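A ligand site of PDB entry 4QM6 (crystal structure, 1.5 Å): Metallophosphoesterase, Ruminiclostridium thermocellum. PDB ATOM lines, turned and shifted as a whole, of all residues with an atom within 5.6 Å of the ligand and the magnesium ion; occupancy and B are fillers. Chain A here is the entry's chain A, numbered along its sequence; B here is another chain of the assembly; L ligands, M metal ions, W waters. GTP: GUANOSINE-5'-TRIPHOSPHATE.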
ATOM      1  N   GLY A  16      27.496 -20.979 -10.554  1.00  0.00           N
ATOM      2  CA  GLY A  16      27.247 -22.099 -11.435  1.00  0.00           C
ATOM      3  C   GLY A  16      25.895 -22.043 -12.100  1.00  0.00           C
ATOM      4  O   GLY A  16      24.948 -21.469 -11.568  1.00  0.00           O
ATOM      5  N   SER A  17      25.824 -22.635 -13.280  1.00  0.00           N
ATOM      6  CA  SER A  17      24.585 -22.782 -14.035  1.00  0.00           C
ATOM      7  C   SER A  17      23.485 -23.482 -13.254  1.00  0.00           C
ATOM      8  O   SER A  17      23.757 -24.247 -12.316  1.00  0.00           O
ATOM      9  CB  SER A  17      24.901 -23.595 -15.290  1.00  0.00           C
ATOM     10  OG  SER A  17      23.754 -23.854 -16.085  1.00  0.00           O
ATOM     11  N   SER A  18      22.237 -23.232 -13.615  1.00  0.00           N
ATOM     12  CA  SER A  18      21.171 -24.121 -13.192  1.00  0.00           C
ATOM     13  C   SER A  18      21.584 -25.542 -13.583  1.00  0.00           C
ATOM     14  O   SER A  18      22.154 -25.766 -14.667  1.00  0.00           O
ATOM     15  CB  SER A  18      19.845 -23.756 -13.856  1.00  0.00           C
ATOM     16  OG  SER A  18      18.793 -24.620 -13.441  1.00  0.00           O
ATOM     17  N   GLY A  19      21.359 -26.482 -12.678  1.00  0.00           N
ATOM     18  CA  GLY A  19      21.739 -27.858 -12.930  1.00  0.00           C
ATOM     19  C   GLY A  19      23.161 -28.249 -12.543  1.00  0.00           C
ATOM     20  O   GLY A  19      23.510 -29.421 -12.669  1.00  0.00           O
ATOM     21  N   SER A  20      23.969 -27.307 -12.079  1.00  0.00           N
ATOM     22  CA  SER A  20      25.370 -27.601 -11.753  1.00  0.00           C
ATOM     23  C   SER A  20      25.551 -28.252 -10.386  1.00  0.00           C
ATOM     24  O   SER A  20      26.667 -28.679 -10.078  1.00  0.00           O
ATOM     25  CB  SER A  20      26.260 -26.357 -11.876  1.00  0.00           C
ATOM     26  OG  SER A  20      25.866 -25.346 -10.969  1.00  0.00           O
ATOM     27  N   GLY A  21      24.484 -28.342  -9.584  1.00  0.00           N
ATOM     28  CA  GLY A  21      24.545 -29.012  -8.285  1.00  0.00           C
ATOM     29  C   GLY A  21      24.776 -28.110  -7.092  1.00  0.00           C
ATOM     30  O   GLY A  21      25.184 -28.581  -6.023  1.00  0.00           O
ATOM     31  N   LYS A  22      24.525 -26.810  -7.248  1.00  0.00           N
ATOM     32  CA  LYS A  22      24.786 -25.849  -6.170  1.00  0.00           C
ATOM     33  C   LYS A  22      24.039 -26.158  -4.881  1.00  0.00           C
ATOM     34  O   LYS A  22      24.639 -26.169  -3.806  1.00  0.00           O
ATOM     35  CB  LYS A  22      24.432 -24.422  -6.600  1.00  0.00           C
ATOM     36  CG  LYS A  22      25.243 -23.888  -7.774  1.00  0.00           C
ATOM     37  CD  LYS A  22      24.869 -22.434  -8.120  1.00  0.00           C
ATOM     38  CE  LYS A  22      23.411 -22.277  -8.512  1.00  0.00           C
ATOM     39  NZ  LYS A  22      23.013 -23.076  -9.706  1.00  0.00           N
ATOM     40  N   SER A  23      22.729 -26.386  -4.971  1.00  0.00           N
ATOM     41  CA  SER A  23      21.926 -26.610  -3.773  1.00  0.00           C
ATOM     42  C   SER A  23      22.287 -27.931  -3.078  1.00  0.00           C
ATOM     43  O   SER A  23      22.311 -28.014  -1.840  1.00  0.00           O
ATOM     44  CB  SER A  23      20.439 -26.600  -4.121  1.00  0.00           C
ATOM     45  OG  SER A  23      20.063 -25.328  -4.661  1.00  0.00           O
ATOM     46  N   THR A  24      22.587 -28.955  -3.866  1.00  0.00           N
ATOM     47  CA  THR A  24      22.999 -30.255  -3.331  1.00  0.00           C
ATOM     48  C   THR A  24      24.342 -30.137  -2.602  1.00  0.00           C
ATOM     49  O   THR A  24      24.556 -30.700  -1.506  1.00  0.00           O
ATOM     50  CB  THR A  24      23.068 -31.288  -4.458  1.00  0.00           C
ATOM     51  OG1 THR A  24      21.754 -31.427  -5.037  1.00  0.00           O
ATOM     52  CG2 THR A  24      23.531 -32.641  -3.951  1.00  0.00           C
ATOM     53  N   PHE A  25      25.253 -29.379  -3.192  1.00  0.00           N
ATOM     54  CA  PHE A  25      26.575 -29.124  -2.616  1.00  0.00           C
ATOM     55  C   PHE A  25      26.432 -28.336  -1.316  1.00  0.00           C
ATOM     56  O   PHE A  25      27.049 -28.674  -0.287  1.00  0.00           O
ATOM     57  CB  PHE A  25      27.392 -28.347  -3.665  1.00  0.00           C
ATOM     58  CG  PHE A  25      28.755 -27.894  -3.208  1.00  0.00           C
ATOM     59  CD1 PHE A  25      28.929 -26.669  -2.590  1.00  0.00           C
ATOM     60  CD2 PHE A  25      29.884 -28.659  -3.502  1.00  0.00           C
ATOM     61  CE1 PHE A  25      30.190 -26.237  -2.225  1.00  0.00           C
ATOM     62  CE2 PHE A  25      31.155 -28.219  -3.156  1.00  0.00           C
ATOM     63  CZ  PHE A  25      31.307 -27.010  -2.524  1.00  0.00           C
ATOM     64  N   ASN A  39      16.201 -18.875  -5.110  1.00  0.00           N
ATOM     65  CA  ASN A  39      14.941 -19.532  -5.406  1.00  0.00           C
ATOM     66  C   ASN A  39      14.029 -19.622  -4.179  1.00  0.00           C
ATOM     67  O   ASN A  39      12.820 -19.394  -4.266  1.00  0.00           O
ATOM     68  CB  ASN A  39      15.159 -20.902  -6.045  1.00  0.00           C
ATOM     69  CG  ASN A  39      15.787 -20.798  -7.426  1.00  0.00           C
ATOM     70  OD1 ASN A  39      15.531 -19.840  -8.152  1.00  0.00           O
ATOM     71  ND2 ASN A  39      16.637 -21.772  -7.771  1.00  0.00           N
ATOM     72  N   ASP A  79      23.369 -19.324  -2.356  1.00  0.00           N
ATOM     73  CA  ASP A  79      22.989 -20.311  -3.346  1.00  0.00           C
ATOM     74  C   ASP A  79      22.139 -19.618  -4.408  1.00  0.00           C
ATOM     75  O   ASP A  79      20.904 -19.517  -4.303  1.00  0.00           O
ATOM     76  CB  ASP A  79      22.244 -21.482  -2.678  1.00  0.00           C
ATOM     77  CG  ASP A  79      21.785 -22.525  -3.665  1.00  0.00           C
ATOM     78  OD1 ASP A  79      22.167 -22.467  -4.856  1.00  0.00           O
ATOM     79  OD2 ASP A  79      20.984 -23.395  -3.264  1.00  0.00           O
ATOM     80  N   THR A  81      22.837 -18.472  -8.977  1.00  0.00           N
ATOM     81  CA  THR A  81      23.774 -18.759 -10.059  1.00  0.00           C
ATOM     82  C   THR A  81      25.028 -17.882 -10.007  1.00  0.00           C
ATOM     83  O   THR A  81      26.132 -18.379 -10.232  1.00  0.00           O
ATOM     84  CB  THR A  81      23.140 -18.669 -11.468  1.00  0.00           C
ATOM     85  OG1 THR A  81      22.644 -17.337 -11.700  1.00  0.00           O
ATOM     86  CG2 THR A  81      22.017 -19.698 -11.627  1.00  0.00           C
ATOM     87  N   ARG A 117      21.368 -33.257 -16.240  1.00  0.00           N
ATOM     88  CA  ARG A 117      20.806 -33.175 -14.903  1.00  0.00           C
ATOM     89  C   ARG A 117      19.451 -32.475 -14.910  1.00  0.00           C
ATOM     90  O   ARG A 117      18.496 -32.937 -14.292  1.00  0.00           O
ATOM     91  CB  ARG A 117      21.778 -32.473 -13.965  1.00  0.00           C
ATOM     92  CG  ARG A 117      22.984 -33.317 -13.627  1.00  0.00           C
ATOM     93  CD  ARG A 117      23.920 -32.567 -12.720  1.00  0.00           C
ATOM     94  NE  ARG A 117      25.137 -33.322 -12.423  1.00  0.00           N
ATOM     95  CZ  ARG A 117      26.141 -32.828 -11.705  1.00  0.00           C
ATOM     96  NH1 ARG A 117      26.043 -31.587 -11.229  1.00  0.00           N
ATOM     97  NH2 ARG A 117      27.228 -33.546 -11.469  1.00  0.00           N
ATOM     98  N   ASN A 118      19.368 -31.372 -15.645  1.00  0.00           N
ATOM     99  CA  ASN A 118      18.137 -30.605 -15.752  1.00  0.00           C
ATOM    100  C   ASN A 118      16.973 -31.434 -16.315  1.00  0.00           C
ATOM    101  O   ASN A 118      15.855 -31.372 -15.807  1.00  0.00           O
ATOM    102  CB  ASN A 118      18.401 -29.365 -16.603  1.00  0.00           C
ATOM    103  CG  ASN A 118      17.163 -28.525 -16.818  1.00  0.00           C
ATOM    104  OD1 ASN A 118      16.617 -27.926 -15.890  1.00  0.00           O
ATOM    105  ND2 ASN A 118      16.743 -28.435 -18.076  1.00  0.00           N
ATOM    106  N   ASN A 120      16.421 -34.573 -16.104  1.00  0.00           N
ATOM    107  CA  ASN A 120      16.001 -35.654 -15.211  1.00  0.00           C
ATOM    108  C   ASN A 120      15.440 -35.160 -13.884  1.00  0.00           C
ATOM    109  O   ASN A 120      15.093 -35.953 -13.013  1.00  0.00           O
ATOM    110  CB  ASN A 120      17.150 -36.636 -14.962  1.00  0.00           C
ATOM    111  CG  ASN A 120      17.570 -37.355 -16.232  1.00  0.00           C
ATOM    112  OD1 ASN A 120      16.775 -38.067 -16.842  1.00  0.00           O
ATOM    113  ND2 ASN A 120      18.825 -37.171 -16.625  1.00  0.00           N
ATOM    114  N   ARG A 121      15.358 -33.845 -13.733  1.00  0.00           N
ATOM    115  CA  ARG A 121      14.822 -33.264 -12.507  1.00  0.00           C
ATOM    116  C   ARG A 121      13.325 -33.382 -12.479  1.00  0.00           C
ATOM    117  O   ARG A 121      12.653 -33.266 -13.508  1.00  0.00           O
ATOM    118  CB  ARG A 121      15.217 -31.795 -12.381  1.00  0.00           C
ATOM    119  CG  ARG A 121      16.688 -31.575 -12.168  1.00  0.00           C
ATOM    120  CD  ARG A 121      17.003 -30.103 -12.041  1.00  0.00           C
ATOM    121  NE  ARG A 121      16.495 -29.551 -10.795  1.00  0.00           N
ATOM    122  CZ  ARG A 121      16.735 -28.314 -10.388  1.00  0.00           C
ATOM    123  NH1 ARG A 121      17.487 -27.516 -11.140  1.00  0.00           N
ATOM    124  NH2 ARG A 121      16.223 -27.865  -9.247  1.00  0.00           N
ATOM    125  N   ASP A 123      11.763 -31.781  -9.623  1.00  0.00           N
ATOM    126  CA  ASP A 123      11.393 -30.664  -8.748  1.00  0.00           C
ATOM    127  C   ASP A 123      11.175 -29.366  -9.513  1.00  0.00           C
ATOM    128  O   ASP A 123      10.172 -28.666  -9.312  1.00  0.00           O
ATOM    129  CB  ASP A 123      12.431 -30.487  -7.622  1.00  0.00           C
ATOM    130  CG  ASP A 123      13.830 -30.225  -8.143  1.00  0.00           C
ATOM    131  OD1 ASP A 123      14.203 -30.760  -9.207  1.00  0.00           O
ATOM    132  OD2 ASP A 123      14.576 -29.472  -7.464  1.00  0.00           O
ATOM    133  N   ARG A 124      12.106 -29.057 -10.411  1.00  0.00           N
ATOM    134  CA  ARG A 124      12.057 -27.839 -11.197  1.00  0.00           C
ATOM    135  C   ARG A 124      13.018 -27.984 -12.372  1.00  0.00           C
ATOM    136  O   ARG A 124      14.067 -28.624 -12.241  1.00  0.00           O
ATOM    137  CB  ARG A 124      12.460 -26.633 -10.336  1.00  0.00           C
ATOM    138  CG  ARG A 124      12.514 -25.301 -11.069  1.00  0.00           C
ATOM    139  CD  ARG A 124      12.717 -24.133 -10.092  1.00  0.00           C
ATOM    140  NE  ARG A 124      13.705 -24.491  -9.094  1.00  0.00           N
ATOM    141  CZ  ARG A 124      15.024 -24.452  -9.293  1.00  0.00           C
ATOM    142  NH1 ARG A 124      15.504 -24.029 -10.463  1.00  0.00           N
ATOM    143  NH2 ARG A 124      15.846 -24.819  -8.324  1.00  0.00           N
ATOM    144  N   VAL A 126      14.593 -25.782 -16.102  1.00  0.00           N
ATOM    145  CA  VAL A 126      14.648 -24.582 -16.954  1.00  0.00           C
ATOM    146  C   VAL A 126      14.814 -25.014 -18.398  1.00  0.00           C
ATOM    147  O   VAL A 126      15.081 -26.172 -18.689  1.00  0.00           O
ATOM    148  CB  VAL A 126      15.807 -23.627 -16.573  1.00  0.00           C
ATOM    149  CG1 VAL A 126      15.648 -23.151 -15.127  1.00  0.00           C
ATOM    150  CG2 VAL A 126      17.191 -24.296 -16.777  1.00  0.00           C
ATOM    151  N   VAL A 162      34.359 -31.811  -7.597  1.00  0.00           N
ATOM    152  CA  VAL A 162      33.287 -31.378  -6.709  1.00  0.00           C
ATOM    153  C   VAL A 162      33.093 -32.384  -5.554  1.00  0.00           C
ATOM    154  O   VAL A 162      32.959 -31.999  -4.388  1.00  0.00           O
ATOM    155  CB  VAL A 162      31.944 -31.215  -7.463  1.00  0.00           C
ATOM    156  CG1 VAL A 162      30.802 -30.956  -6.489  1.00  0.00           C
ATOM    157  CG2 VAL A 162      32.027 -30.081  -8.478  1.00  0.00           C
ATOM    158  O5'   C B   1      18.278 -21.638 -10.137  1.00  0.00           O
ATOM    159  C5'   C B   1      17.660 -21.376 -11.404  1.00  0.00           C
ATOM    160  C4'   C B   1      18.287 -20.153 -11.999  1.00  0.00           C
ATOM    161  O4'   C B   1      17.912 -20.023 -13.407  1.00  0.00           O
ATOM    162  C3'   C B   1      17.871 -18.840 -11.313  1.00  0.00           C
ATOM    163  O3'   C B   1      19.027 -18.003 -11.260  1.00  0.00           O
ATOM    164  C2'   C B   1      16.876 -18.259 -12.312  1.00  0.00           C
ATOM    165  O2'   C B   1      16.668 -16.871 -12.225  1.00  0.00           O
ATOM    166  C1'   C B   1      17.530 -18.686 -13.624  1.00  0.00           C
ATOM    167  N1    C B   1      16.657 -18.561 -14.786  1.00  0.00           N
ATOM    168  C2    C B   1      17.075 -17.740 -15.837  1.00  0.00           C
ATOM    169  O2    C B   1      18.217 -17.234 -15.832  1.00  0.00           O
ATOM    170  N3    C B   1      16.219 -17.555 -16.884  1.00  0.00           N
ATOM    171  C4    C B   1      15.015 -18.153 -16.849  1.00  0.00           C
ATOM    172  N4    C B   1      14.163 -17.960 -17.870  1.00  0.00           N
ATOM    173  C5    C B   1      14.571 -18.957 -15.778  1.00  0.00           C
ATOM    174  C6    C B   1      15.435 -19.138 -14.762  1.00  0.00           C
HETATM  175  PG  GTP L   1      19.291 -24.560  -9.783  1.00  0.00           P
HETATM  176  O1G GTP L   1      18.264 -24.754 -10.861  1.00  0.00           O
HETATM  177  O2G GTP L   1      20.193 -23.361 -10.057  1.00  0.00           O
HETATM  178  O3G GTP L   1      18.630 -24.473  -8.421  1.00  0.00           O
HETATM  179  O3B GTP L   1      20.271 -25.892  -9.845  1.00  0.00           O
HETATM  180  PB  GTP L   1      21.450 -26.340  -8.816  1.00  0.00           P
HETATM  181  O1B GTP L   1      21.034 -25.926  -7.418  1.00  0.00           O
HETATM  182  O2B GTP L   1      22.777 -25.794  -9.258  1.00  0.00           O
HETATM  183  O3A GTP L   1      21.471 -27.961  -8.898  1.00  0.00           O
HETATM  184  PA  GTP L   1      20.746 -28.987  -7.873  1.00  0.00           P
HETATM  185  O1A GTP L   1      19.279 -28.683  -7.633  1.00  0.00           O
HETATM  186  O2A GTP L   1      21.599 -29.148  -6.640  1.00  0.00           O
HETATM  187  O5' GTP L   1      20.901 -30.325  -8.735  1.00  0.00           O
HETATM  188  C5' GTP L   1      20.231 -30.487  -9.976  1.00  0.00           C
HETATM  189  C4' GTP L   1      20.138 -31.990 -10.188  1.00  0.00           C
HETATM  190  O4' GTP L   1      21.465 -32.491 -10.276  1.00  0.00           O
HETATM  191  C3' GTP L   1      19.471 -32.656  -8.995  1.00  0.00           C
HETATM  192  O3' GTP L   1      18.506 -33.556  -9.459  1.00  0.00           O
HETATM  193  C2' GTP L   1      20.600 -33.395  -8.301  1.00  0.00           C
HETATM  194  O2' GTP L   1      20.189 -34.635  -7.771  1.00  0.00           O
HETATM  195  C1' GTP L   1      21.679 -33.559  -9.359  1.00  0.00           C
HETATM  196  N9  GTP L   1      23.000 -33.401  -8.735  1.00  0.00           N
HETATM  197  C8  GTP L   1      23.414 -32.347  -7.959  1.00  0.00           C
HETATM  198  N7  GTP L   1      24.690 -32.571  -7.549  1.00  0.00           N
HETATM  199  C5  GTP L   1      25.088 -33.753  -8.070  1.00  0.00           C
HETATM  200  C6  GTP L   1      26.279 -34.454  -7.961  1.00  0.00           C
HETATM  201  O6  GTP L   1      27.214 -33.979  -7.311  1.00  0.00           O
HETATM  202  N1  GTP L   1      26.419 -35.668  -8.605  1.00  0.00           N
HETATM  203  C2  GTP L   1      25.361 -36.180  -9.334  1.00  0.00           C
HETATM  204  N2  GTP L   1      25.500 -37.349  -9.953  1.00  0.00           N
HETATM  205  N3  GTP L   1      24.180 -35.485  -9.435  1.00  0.00           N
HETATM  206  C4  GTP L   1      24.047 -34.285  -8.810  1.00  0.00           C
HETATM  207 MG    MG M   1      19.304 -24.815  -6.533  1.00  0.00          MG
HETATM  208  O   HOH W   1      30.066 -34.581  -8.064  1.00  0.00           O
HETATM  209  O   HOH W   2      18.732 -34.775 -12.237  1.00  0.00           O
HETATM  210  O   HOH W   3      29.100 -36.867  -8.960  1.00  0.00           O
HETATM  211  O   HOH W   4      19.258 -36.596  -8.989  1.00  0.00           O
HETATM  212  O   HOH W   5      17.436 -30.466  -7.107  1.00  0.00           O
HETATM  213  O   HOH W   6      18.173 -26.587  -6.524  1.00  0.00           O
HETATM  214  O   HOH W   7      19.829 -33.266  -4.922  1.00  0.00           O
HETATM  215  O   HOH W   8      29.602 -34.470  -5.404  1.00  0.00           O
HETATM  216  O   HOH W   9      26.768 -30.963  -6.165  1.00  0.00           O
HETATM  217  O   HOH W  10      17.709 -23.757  -5.643  1.00  0.00           O
HETATM  218  O   HOH W  11      29.185 -32.552  -9.777  1.00  0.00           O
HETATM  219  O   HOH W  12      20.346 -23.106  -6.521  1.00  0.00           O
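The magnesium ion is bound by water W12 (2.0 Å), O3G of the ligand (2.0 Å), OG of Ser 23 (2.1 Å), water W6 (2.1 Å), water W10 (2.1 Å) and O1B of the ligand (2.2 Å).
Asp 79 touches the magnesium ion (OD2 to MG, 3.9 Å). NH2 of Arg 124 touches the magnesium ion (3.9 Å). Three residues have an atom within 4 Å of the magnesium ion: Ser 23, Asp 79 and Arg 124.
The side-chain amino group of Lys 22 is in hydrogen-bond range of the backbone carbonyl oxygen of Gly 16, at 3.1 Å. O5' of C 1 of chain B lies within hydrogen-bond range of ND2 of Asn 39. OG of Ser 23 sits close to OD2 of Asp 79, at 2.6 Å. O of Ser 20 is in hydrogen-bond range of NH1 of Arg 117, at 3.2 Å. The guanidinium group of Arg 121 lies within hydrogen-bond range of the backbone carbonyl oxygen of Arg 124, at 3.0 Å. The side-chain amide nitrogen of Asn 39 sits close to the guanidinium group of Arg 124 (3.2 Å). O of Ser 17 is in hydrogen-bond range of OG of Ser 20 (2.7 Å). The backbone carbonyl oxygen (O) of Ser 17 lies within hydrogen-bond range of the side-chain amino group (NZ) of Lys 22, at 3.0 Å.
Residues that only touch the ligand: Arg 117 and Ser 17.
Water W10 lies within hydrogen-bond range of the side-chain amide nitrogen (ND2) of Asn 39 and the guanidinium group (NH2) of Arg 124. Water W6 bridges O1A of the ligand (2.6 Å) and NH2 of Arg 124 (3.4 Å). Water W5 bridges an oxygen (O1A) of the ligand (2.6 Å) and the side-chain carboxylate of Asp 123 (3.0 Å). Water W9 lies within hydrogen-bond range of O of Gly 21 (2.9 Å) and N7 of the ligand (3.0 Å). Water W7 bridges the side-chain hydroxyl (OG1) of Thr 24 and an oxygen (O2') of the ligand. Water W11 bridges the guanidinium group (NH2) of Arg 117 (2.8 Å) and an oxygen (O6) of the ligand (3.5 Å).
The backbone NH of Thr 24 is in hydrogen-bond range of an oxygen (O2A) of the ligand, 3.0 Å away. An oxygen (O2B) of the ligand lies within hydrogen-bond range of the backbone NH of Gly 21 (3.1 Å). O5' of C 1 of chain B lies close to an oxygen (O2G) of the ligand (2.6 Å). N of Gly 19 lies within hydrogen-bond range of O3B of the ligand, at 3.1 Å. O3G of the ligand lies close to ND2 of Asn 39 (3.4 Å). The backbone NH (N) of Lys 22 lies within hydrogen-bond range of an oxygen (O2B) of the ligand. The side-chain hydroxyl of Ser 18 lies within hydrogen-bond range of an oxygen (O1G) of the ligand (2.6 Å). An oxygen (O1G) of the ligand lies within salt-bridge range of the guanidinium group (NH1) of Arg 121, 2.9 Å away. O1G of the ligand is in salt-bridge range of NH1 of Arg 124 (2.9 Å). The backbone NH (N) of Ser 23 is in hydrogen-bond range of an oxygen (O2A) of the ligand, at 3.4 Å. The backbone NH (N) of Ser 20 is in hydrogen-bond range of an oxygen (O2B) of the ligand (3.4 Å). The side-chain hydroxyl of Thr 24 is in hydrogen-bond range of an oxygen (O2A) of the ligand (2.8 Å). NZ of Lys 22 is in salt-bridge range of O2B of the ligand (2.8 Å).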
